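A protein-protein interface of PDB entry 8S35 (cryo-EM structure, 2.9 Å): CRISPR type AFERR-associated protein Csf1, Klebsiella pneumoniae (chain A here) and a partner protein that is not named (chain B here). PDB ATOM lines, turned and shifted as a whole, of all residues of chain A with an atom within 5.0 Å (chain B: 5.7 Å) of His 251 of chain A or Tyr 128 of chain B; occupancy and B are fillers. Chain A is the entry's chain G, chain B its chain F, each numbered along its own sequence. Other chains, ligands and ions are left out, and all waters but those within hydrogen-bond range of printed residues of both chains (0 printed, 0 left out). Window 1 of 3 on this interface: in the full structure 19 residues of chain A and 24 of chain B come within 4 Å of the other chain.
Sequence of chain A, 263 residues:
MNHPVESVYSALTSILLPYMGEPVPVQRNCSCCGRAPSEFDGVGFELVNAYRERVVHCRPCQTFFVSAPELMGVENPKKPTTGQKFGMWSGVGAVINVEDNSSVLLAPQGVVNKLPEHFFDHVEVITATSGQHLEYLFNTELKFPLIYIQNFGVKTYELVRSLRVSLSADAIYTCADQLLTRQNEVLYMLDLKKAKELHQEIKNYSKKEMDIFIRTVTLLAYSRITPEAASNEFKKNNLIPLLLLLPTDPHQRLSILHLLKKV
Along chain B the printed residues that touch a printed residue of chain A span positions 78 to 224.
Of the 9 printed residues of chain A, 6 touch a printed residue of chain B.
Printed residues of chain A that touch a printed residue of chain B: Val 186, Leu 187, Asp 249, Pro 250, His 251 and Leu 254.
Along chain A the printed residues that touch a printed residue of chain B span positions 186 to 254.
Among the printed residues, no Asp or Glu carboxylate lies within 4 Å of a Lys or Arg side-chain nitrogen of the other chain.
The side-chain carboxylate (OD2) of Asp 249 of chain A sits at hydrogen-bond distance from the side-chain hydroxyl (OH) of Tyr 128 of chain B (2.7 Å).
The backbone carbonyl oxygen (O) of His 251 of chain A sits at hydrogen-bond distance from the side-chain hydroxyl (OG) of Ser 255 of chain A, 3.1 Å away.
The side-chain amide oxygen (OE1) of Gln 252 of chain A lies close to the backbone carbonyl oxygen (O) of Val 186 of chain A (2.9 Å).
The side-chain carboxylate (OD1) of Asp 249 of chain A is in hydrogen-bond range of the backbone NH (N) of Gln 252 of chain A (3.2 Å).
The backbone NH (N) of Ser 129 of chain B lies within hydrogen-bond range of the backbone carbonyl oxygen (O) of Gly 79 of chain B, 2.7 Å away.
The side-chain hydroxyl of Thr 81 of chain B sits at hydrogen-bond distance from the side-chain hydroxyl of Ser 129 of chain B, 3.4 Å away.
O of Thr 81 of chain B is in hydrogen-bond range of N of Ala 127 of chain B.
Of the printed residues of chain B, Leu 187 of chain A touches Pro 126 (3.6 Å).
Of the printed residues of chain B, Asp 249 of chain A touches Tyr 128 (2.7 Å) and Val 224 (3.0 Å).
Val 17 of chain B touches none of the printed residues of chain A.
Val 18 of chain B touches none of the printed residues of chain A.
Of the printed residues of chain A, Ile 78 of chain B touches Pro 250 (3.7 Å).
Printed residues of chain A within 4 Å of Gly 79 of chain B: Pro 250.
Of the printed residues of chain A, Thr 81 of chain B touches His 251 (3.9 Å).
The nearest residue of chain B that does not touch His 251 of chain A is Thr 82 of chain B (4.5 Å).
The nearest printed residue of chain A that does not touch Ala 127 of chain B is Pro 250 of chain A (5.6 Å).
Among the printed residues, merely in contact across the chains: Asp 249 of chain A with Val 224 of chain B (3.0 Å), Val 186 of chain A with Tyr 128 of chain B (3.3 Å), Val 186 of chain A with Pro 126 of chain B (3.4 Å), Leu 254 of chain A with Ala 80 of chain B (3.5 Å), Pro 250 of chain A with Tyr 128 of chain B (3.6 Å), His 251 of chain A with Pro 126 of chain B (3.6 Å), His 251 of chain A with Ala 80 of chain B (3.6 Å), Leu 187 of chain A with Pro 126 of chain B (3.6 Å), His 251 of chain A with Tyr 128 of chain B (3.7 Å), Pro 250 of chain A with Ile 78 of chain B (3.7 Å), His 251 of chain A with Ala 127 of chain B (3.8 Å), His 251 of chain A with Thr 81 of chain B (3.9 Å), Pro 250 of chain A with Val 224 of chain B (3.9 Å) and Pro 250 of chain A with Gly 79 of chain B (3.97 Å).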
ATOM      1  N   VAL A 186      18.820  15.495   1.522  1.00  0.00           N
ATOM      2  CA  VAL A 186      18.263  16.599   0.748  1.00  0.00           C
ATOM      3  C   VAL A 186      18.982  17.896   1.085  1.00  0.00           C
ATOM      4  O   VAL A 186      19.152  18.765   0.221  1.00  0.00           O
ATOM      5  CB  VAL A 186      16.742  16.702   0.986  1.00  0.00           C
ATOM      6  CG1 VAL A 186      16.449  17.291   2.348  1.00  0.00           C
ATOM      7  CG2 VAL A 186      16.083  17.519  -0.113  1.00  0.00           C
ATOM      8  N   LEU A 187      19.422  18.048   2.335  1.00  0.00           N
ATOM      9  CA  LEU A 187      20.187  19.217   2.748  1.00  0.00           C
ATOM     10  C   LEU A 187      21.647  19.137   2.335  1.00  0.00           C
ATOM     11  O   LEU A 187      22.360  20.141   2.447  1.00  0.00           O
ATOM     12  CB  LEU A 187      20.107  19.392   4.266  1.00  0.00           C
ATOM     13  CG  LEU A 187      19.219  20.535   4.753  1.00  0.00           C
ATOM     14  CD1 LEU A 187      17.808  20.391   4.213  1.00  0.00           C
ATOM     15  CD2 LEU A 187      19.215  20.586   6.272  1.00  0.00           C
ATOM     16  N   ASP A 249      10.534  20.221  -4.030  1.00  0.00           N
ATOM     17  CA  ASP A 249      11.012  20.182  -2.654  1.00  0.00           C
ATOM     18  C   ASP A 249      11.409  21.584  -2.195  1.00  0.00           C
ATOM     19  O   ASP A 249      12.202  22.247  -2.872  1.00  0.00           O
ATOM     20  CB  ASP A 249      12.199  19.231  -2.544  1.00  0.00           C
ATOM     21  CG  ASP A 249      12.600  18.957  -1.109  1.00  0.00           C
ATOM     22  OD1 ASP A 249      12.883  19.921  -0.367  1.00  0.00           O
ATOM     23  OD2 ASP A 249      12.645  17.771  -0.724  1.00  0.00           O
ATOM     24  N   PRO A 250      10.895  22.072  -1.059  1.00  0.00           N
ATOM     25  CA  PRO A 250      11.285  23.420  -0.622  1.00  0.00           C
ATOM     26  C   PRO A 250      12.719  23.496  -0.141  1.00  0.00           C
ATOM     27  O   PRO A 250      13.367  24.534  -0.321  1.00  0.00           O
ATOM     28  CB  PRO A 250      10.295  23.718   0.508  1.00  0.00           C
ATOM     29  CG  PRO A 250      10.002  22.395   1.080  1.00  0.00           C
ATOM     30  CD  PRO A 250       9.991  21.439  -0.083  1.00  0.00           C
ATOM     31  N   HIS A 251      13.242  22.429   0.462  1.00  0.00           N
ATOM     32  CA  HIS A 251      14.622  22.466   0.928  1.00  0.00           C
ATOM     33  C   HIS A 251      15.586  22.509  -0.247  1.00  0.00           C
ATOM     34  O   HIS A 251      16.591  23.228  -0.207  1.00  0.00           O
ATOM     35  CB  HIS A 251      14.916  21.265   1.821  1.00  0.00           C
ATOM     36  CG  HIS A 251      14.685  21.528   3.276  1.00  0.00           C
ATOM     37  ND1 HIS A 251      15.450  22.415   4.001  1.00  0.00           N
ATOM     38  CD2 HIS A 251      13.771  21.027   4.138  1.00  0.00           C
ATOM     39  CE1 HIS A 251      15.022  22.441   5.250  1.00  0.00           C
ATOM     40  NE2 HIS A 251      14.002  21.609   5.359  1.00  0.00           N
ATOM     41  N   GLN A 252      15.307  21.742  -1.301  1.00  0.00           N
ATOM     42  CA  GLN A 252      16.150  21.818  -2.485  1.00  0.00           C
ATOM     43  C   GLN A 252      16.044  23.192  -3.125  1.00  0.00           C
ATOM     44  O   GLN A 252      17.033  23.718  -3.645  1.00  0.00           O
ATOM     45  CB  GLN A 252      15.745  20.744  -3.496  1.00  0.00           C
ATOM     46  CG  GLN A 252      16.209  19.284  -3.262  1.00  0.00           C
ATOM     47  CD  GLN A 252      17.673  19.056  -2.870  1.00  0.00           C
ATOM     48  OE1 GLN A 252      18.363  19.916  -2.337  1.00  0.00           O
ATOM     49  NE2 GLN A 252      18.126  17.839  -3.103  1.00  0.00           N
ATOM     50  N   ARG A 253      14.845  23.777  -3.112  1.00  0.00           N
ATOM     51  CA  ARG A 253      14.683  25.143  -3.593  1.00  0.00           C
ATOM     52  C   ARG A 253      15.592  26.090  -2.826  1.00  0.00           C
ATOM     53  O   ARG A 253      16.290  26.920  -3.417  1.00  0.00           O
ATOM     54  CB  ARG A 253      13.226  25.582  -3.455  1.00  0.00           C
ATOM     55  CG  ARG A 253      12.310  25.111  -4.564  1.00  0.00           C
ATOM     56  CD  ARG A 253      10.898  25.620  -4.335  1.00  0.00           C
ATOM     57  NE  ARG A 253       9.948  25.083  -5.303  1.00  0.00           N
ATOM     58  CZ  ARG A 253       8.677  25.451  -5.396  1.00  0.00           C
ATOM     59  NH1 ARG A 253       8.158  26.365  -4.592  1.00  0.00           N
ATOM     60  NH2 ARG A 253       7.904  24.883  -6.315  1.00  0.00           N
ATOM     61  N   LEU A 254      15.599  25.976  -1.498  1.00  0.00           N
ATOM     62  CA  LEU A 254      16.450  26.841  -0.689  1.00  0.00           C
ATOM     63  C   LEU A 254      17.922  26.604  -0.995  1.00  0.00           C
ATOM     64  O   LEU A 254      18.706  27.555  -1.073  1.00  0.00           O
ATOM     65  CB  LEU A 254      16.167  26.611   0.793  1.00  0.00           C
ATOM     66  CG  LEU A 254      14.792  27.078   1.266  1.00  0.00           C
ATOM     67  CD1 LEU A 254      14.375  26.321   2.511  1.00  0.00           C
ATOM     68  CD2 LEU A 254      14.803  28.572   1.530  1.00  0.00           C
ATOM     69  N   SER A 255      18.315  25.343  -1.163  1.00  0.00           N
ATOM     70  CA  SER A 255      19.713  25.034  -1.445  1.00  0.00           C
ATOM     71  C   SER A 255      20.153  25.639  -2.773  1.00  0.00           C
ATOM     72  O   SER A 255      21.208  26.281  -2.862  1.00  0.00           O
ATOM     73  CB  SER A 255      19.914  23.520  -1.455  1.00  0.00           C
ATOM     74  OG  SER A 255      19.632  22.967  -0.182  1.00  0.00           O
ATOM     75  N   SER B  13      -2.039  17.796   8.107  1.00  0.00           N
ATOM     76  CA  SER B  13      -0.731  17.702   8.736  1.00  0.00           C
ATOM     77  C   SER B  13      -0.682  18.622   9.943  1.00  0.00           C
ATOM     78  O   SER B  13      -1.084  19.787   9.866  1.00  0.00           O
ATOM     79  CB  SER B  13       0.368  18.075   7.749  1.00  0.00           C
ATOM     80  OG  SER B  13       1.645  17.767   8.276  1.00  0.00           O
ATOM     81  N   THR B  15       2.318  18.388  12.253  1.00  0.00           N
ATOM     82  CA  THR B  15       3.730  18.617  12.504  1.00  0.00           C
ATOM     83  C   THR B  15       4.517  18.356  11.232  1.00  0.00           C
ATOM     84  O   THR B  15       4.016  17.708  10.307  1.00  0.00           O
ATOM     85  CB  THR B  15       4.249  17.713  13.628  1.00  0.00           C
ATOM     86  OG1 THR B  15       4.191  16.344  13.213  1.00  0.00           O
ATOM     87  CG2 THR B  15       3.413  17.900  14.865  1.00  0.00           C
ATOM     88  N   PRO B  16       5.745  18.870  11.139  1.00  0.00           N
ATOM     89  CA  PRO B  16       6.536  18.650   9.923  1.00  0.00           C
ATOM     90  C   PRO B  16       6.752  17.169   9.654  1.00  0.00           C
ATOM     91  O   PRO B  16       6.930  16.369  10.574  1.00  0.00           O
ATOM     92  CB  PRO B  16       7.858  19.362  10.225  1.00  0.00           C
ATOM     93  CG  PRO B  16       7.543  20.333  11.287  1.00  0.00           C
ATOM     94  CD  PRO B  16       6.466  19.712  12.109  1.00  0.00           C
ATOM     95  N   VAL B  17       6.728  16.814   8.374  1.00  0.00           N
ATOM     96  CA  VAL B  17       6.944  15.446   7.921  1.00  0.00           C
ATOM     97  C   VAL B  17       8.387  15.321   7.462  1.00  0.00           C
ATOM     98  O   VAL B  17       8.846  16.105   6.623  1.00  0.00           O
ATOM     99  CB  VAL B  17       5.974  15.078   6.787  1.00  0.00           C
ATOM    100  CG1 VAL B  17       6.385  13.765   6.134  1.00  0.00           C
ATOM    101  CG2 VAL B  17       4.550  15.000   7.313  1.00  0.00           C
ATOM    102  N   VAL B  18       9.098  14.335   7.997  1.00  0.00           N
ATOM    103  CA  VAL B  18      10.495  14.096   7.660  1.00  0.00           C
ATOM    104  C   VAL B  18      10.530  12.909   6.707  1.00  0.00           C
ATOM    105  O   VAL B  18      10.198  11.784   7.091  1.00  0.00           O
ATOM    106  CB  VAL B  18      11.342  13.827   8.911  1.00  0.00           C
ATOM    107  CG1 VAL B  18      12.761  13.441   8.519  1.00  0.00           C
ATOM    108  CG2 VAL B  18      11.350  15.038   9.833  1.00  0.00           C
ATOM    109  N   ILE B  19      10.952  13.152   5.474  1.00  0.00           N
ATOM    110  CA  ILE B  19      10.980  12.122   4.444  1.00  0.00           C
ATOM    111  C   ILE B  19      12.355  11.474   4.436  1.00  0.00           C
ATOM    112  O   ILE B  19      13.376  12.163   4.339  1.00  0.00           O
ATOM    113  CB  ILE B  19      10.641  12.710   3.065  1.00  0.00           C
ATOM    114  CG1 ILE B  19       9.220  13.282   3.075  1.00  0.00           C
ATOM    115  CG2 ILE B  19      10.816  11.639   1.988  1.00  0.00           C
ATOM    116  CD1 ILE B  19       8.839  14.030   1.821  1.00  0.00           C
ATOM    117  N   PHE B  70       1.923  16.068  -0.881  1.00  0.00           N
ATOM    118  CA  PHE B  70       1.553  17.153   0.018  1.00  0.00           C
ATOM    119  C   PHE B  70       0.405  17.953  -0.582  1.00  0.00           C
ATOM    120  O   PHE B  70       0.559  18.594  -1.625  1.00  0.00           O
ATOM    121  CB  PHE B  70       2.763  18.039   0.286  1.00  0.00           C
ATOM    122  CG  PHE B  70       3.837  17.358   1.078  1.00  0.00           C
ATOM    123  CD1 PHE B  70       3.780  17.320   2.457  1.00  0.00           C
ATOM    124  CD2 PHE B  70       4.903  16.755   0.441  1.00  0.00           C
ATOM    125  CE1 PHE B  70       4.764  16.694   3.186  1.00  0.00           C
ATOM    126  CE2 PHE B  70       5.891  16.127   1.165  1.00  0.00           C
ATOM    127  CZ  PHE B  70       5.821  16.097   2.539  1.00  0.00           C
ATOM    128  N   ILE B  78       3.856  24.186   0.815  1.00  0.00           N
ATOM    129  CA  ILE B  78       4.931  23.337   1.305  1.00  0.00           C
ATOM    130  C   ILE B  78       6.003  24.222   1.920  1.00  0.00           C
ATOM    131  O   ILE B  78       6.495  25.164   1.287  1.00  0.00           O
ATOM    132  CB  ILE B  78       5.475  22.459   0.166  1.00  0.00           C
ATOM    133  CG1 ILE B  78       6.361  21.338   0.714  1.00  0.00           C
ATOM    134  CG2 ILE B  78       6.253  23.288  -0.847  1.00  0.00           C
ATOM    135  CD1 ILE B  78       5.601  20.202   1.340  1.00  0.00           C
ATOM    136  N   GLY B  79       6.344  23.945   3.174  1.00  0.00           N
ATOM    137  CA  GLY B  79       7.300  24.749   3.910  1.00  0.00           C
ATOM    138  C   GLY B  79       8.456  23.906   4.404  1.00  0.00           C
ATOM    139  O   GLY B  79       8.304  22.716   4.677  1.00  0.00           O
ATOM    140  N   ALA B  80       9.615  24.542   4.532  1.00  0.00           N
ATOM    141  CA  ALA B  80      10.848  23.884   4.946  1.00  0.00           C
ATOM    142  C   ALA B  80      11.095  24.183   6.419  1.00  0.00           C
ATOM    143  O   ALA B  80      11.459  25.308   6.775  1.00  0.00           O
ATOM    144  CB  ALA B  80      12.018  24.351   4.087  1.00  0.00           C
ATOM    145  N   THR B  81      10.895  23.180   7.271  1.00  0.00           N
ATOM    146  CA  THR B  81      11.125  23.303   8.701  1.00  0.00           C
ATOM    147  C   THR B  81      11.970  22.120   9.141  1.00  0.00           C
ATOM    148  O   THR B  81      11.891  21.040   8.560  1.00  0.00           O
ATOM    149  CB  THR B  81       9.809  23.337   9.488  1.00  0.00           C
ATOM    150  OG1 THR B  81       8.955  24.353   8.949  1.00  0.00           O
ATOM    151  CG2 THR B  81      10.068  23.627  10.960  1.00  0.00           C
ATOM    152  N   THR B  82      12.789  22.329  10.160  1.00  0.00           N
ATOM    153  CA  THR B  82      13.737  21.318  10.607  1.00  0.00           C
ATOM    154  C   THR B  82      13.172  20.581  11.812  1.00  0.00           C
ATOM    155  O   THR B  82      12.904  21.193  12.850  1.00  0.00           O
ATOM    156  CB  THR B  82      15.088  21.943  10.952  1.00  0.00           C
ATOM    157  OG1 THR B  82      14.927  22.877  12.022  1.00  0.00           O
ATOM    158  CG2 THR B  82      15.671  22.655   9.742  1.00  0.00           C
ATOM    159  N   ARG B 125      16.943  17.357  11.287  1.00  0.00           N
ATOM    160  CA  ARG B 125      16.587  16.707  10.040  1.00  0.00           C
ATOM    161  C   ARG B 125      15.700  17.636   9.228  1.00  0.00           C
ATOM    162  O   ARG B 125      14.962  18.436   9.802  1.00  0.00           O
ATOM    163  CB  ARG B 125      15.846  15.388  10.292  1.00  0.00           C
ATOM    164  CG  ARG B 125      16.623  14.403  11.140  1.00  0.00           C
ATOM    165  CD  ARG B 125      15.914  13.067  11.211  1.00  0.00           C
ATOM    166  NE  ARG B 125      16.690  12.077  11.946  1.00  0.00           N
ATOM    167  CZ  ARG B 125      16.858  12.075  13.262  1.00  0.00           C
ATOM    168  NH1 ARG B 125      16.305  12.997  14.034  1.00  0.00           N
ATOM    169  NH2 ARG B 125      17.597  11.121  13.818  1.00  0.00           N
ATOM    170  N   PRO B 126      15.755  17.573   7.902  1.00  0.00           N
ATOM    171  CA  PRO B 126      14.794  18.345   7.112  1.00  0.00           C
ATOM    172  C   PRO B 126      13.395  17.799   7.309  1.00  0.00           C
ATOM    173  O   PRO B 126      13.198  16.629   7.643  1.00  0.00           O
ATOM    174  CB  PRO B 126      15.263  18.158   5.666  1.00  0.00           C
ATOM    175  CG  PRO B 126      16.484  17.355   5.717  1.00  0.00           C
ATOM    176  CD  PRO B 126      16.628  16.751   7.055  1.00  0.00           C
ATOM    177  N   ALA B 127      12.412  18.665   7.100  1.00  0.00           N
ATOM    178  CA  ALA B 127      11.021  18.272   7.218  1.00  0.00           C
ATOM    179  C   ALA B 127      10.199  19.250   6.402  1.00  0.00           C
ATOM    180  O   ALA B 127      10.525  20.439   6.320  1.00  0.00           O
ATOM    181  CB  ALA B 127      10.552  18.251   8.675  1.00  0.00           C
ATOM    182  N   TYR B 128       9.136  18.739   5.800  1.00  0.00           N
ATOM    183  CA  TYR B 128       8.296  19.516   4.905  1.00  0.00           C
ATOM    184  C   TYR B 128       6.950  19.738   5.576  1.00  0.00           C
ATOM    185  O   TYR B 128       6.255  18.776   5.919  1.00  0.00           O
ATOM    186  CB  TYR B 128       8.157  18.794   3.570  1.00  0.00           C
ATOM    187  CG  TYR B 128       9.489  18.282   3.087  1.00  0.00           C
ATOM    188  CD1 TYR B 128      10.450  19.154   2.606  1.00  0.00           C
ATOM    189  CD2 TYR B 128       9.800  16.935   3.145  1.00  0.00           C
ATOM    190  CE1 TYR B 128      11.675  18.699   2.175  1.00  0.00           C
ATOM    191  CE2 TYR B 128      11.022  16.469   2.716  1.00  0.00           C
ATOM    192  CZ  TYR B 128      11.957  17.354   2.233  1.00  0.00           C
ATOM    193  OH  TYR B 128      13.179  16.894   1.803  1.00  0.00           O
ATOM    194  N   SER B 129       6.596  21.004   5.764  1.00  0.00           N
ATOM    195  CA  SER B 129       5.411  21.409   6.513  1.00  0.00           C
ATOM    196  C   SER B 129       4.365  21.914   5.525  1.00  0.00           C
ATOM    197  O   SER B 129       4.309  23.103   5.211  1.00  0.00           O
ATOM    198  CB  SER B 129       5.762  22.476   7.539  1.00  0.00           C
ATOM    199  OG  SER B 129       6.353  23.601   6.914  1.00  0.00           O
ATOM    200  N   ALA B 130       3.545  21.004   5.043  1.00  0.00           N
ATOM    201  CA  ALA B 130       2.417  21.320   4.189  1.00  0.00           C
ATOM    202  C   ALA B 130       1.142  21.305   5.010  1.00  0.00           C
ATOM    203  O   ALA B 130       1.088  20.679   6.070  1.00  0.00           O
ATOM    204  CB  ALA B 130       2.304  20.303   3.054  1.00  0.00           C
ATOM    205  N   LEU B 133      -1.644  16.229   3.966  1.00  0.00           N
ATOM    206  CA  LEU B 133      -0.972  15.085   3.374  1.00  0.00           C
ATOM    207  C   LEU B 133      -2.014  14.246   2.653  1.00  0.00           C
ATOM    208  O   LEU B 133      -3.180  14.204   3.059  1.00  0.00           O
ATOM    209  CB  LEU B 133      -0.261  14.241   4.432  1.00  0.00           C
ATOM    210  CG  LEU B 133       0.448  14.998   5.555  1.00  0.00           C
ATOM    211  CD1 LEU B 133       1.040  14.015   6.537  1.00  0.00           C
ATOM    212  CD2 LEU B 133       1.530  15.914   5.010  1.00  0.00           C
ATOM    213  N   VAL B 224       9.254  14.846  -2.560  1.00  0.00           N
ATOM    214  CA  VAL B 224       8.338  15.903  -2.150  1.00  0.00           C
ATOM    215  C   VAL B 224       7.489  16.255  -3.362  1.00  0.00           C
ATOM    216  O   VAL B 224       7.948  16.944  -4.279  1.00  0.00           O
ATOM    217  CB  VAL B 224       9.081  17.130  -1.616  1.00  0.00           C
ATOM    218  CG1 VAL B 224       8.100  18.262  -1.345  1.00  0.00           C
ATOM    219  CG2 VAL B 224       9.847  16.773  -0.363  1.00  0.00           C
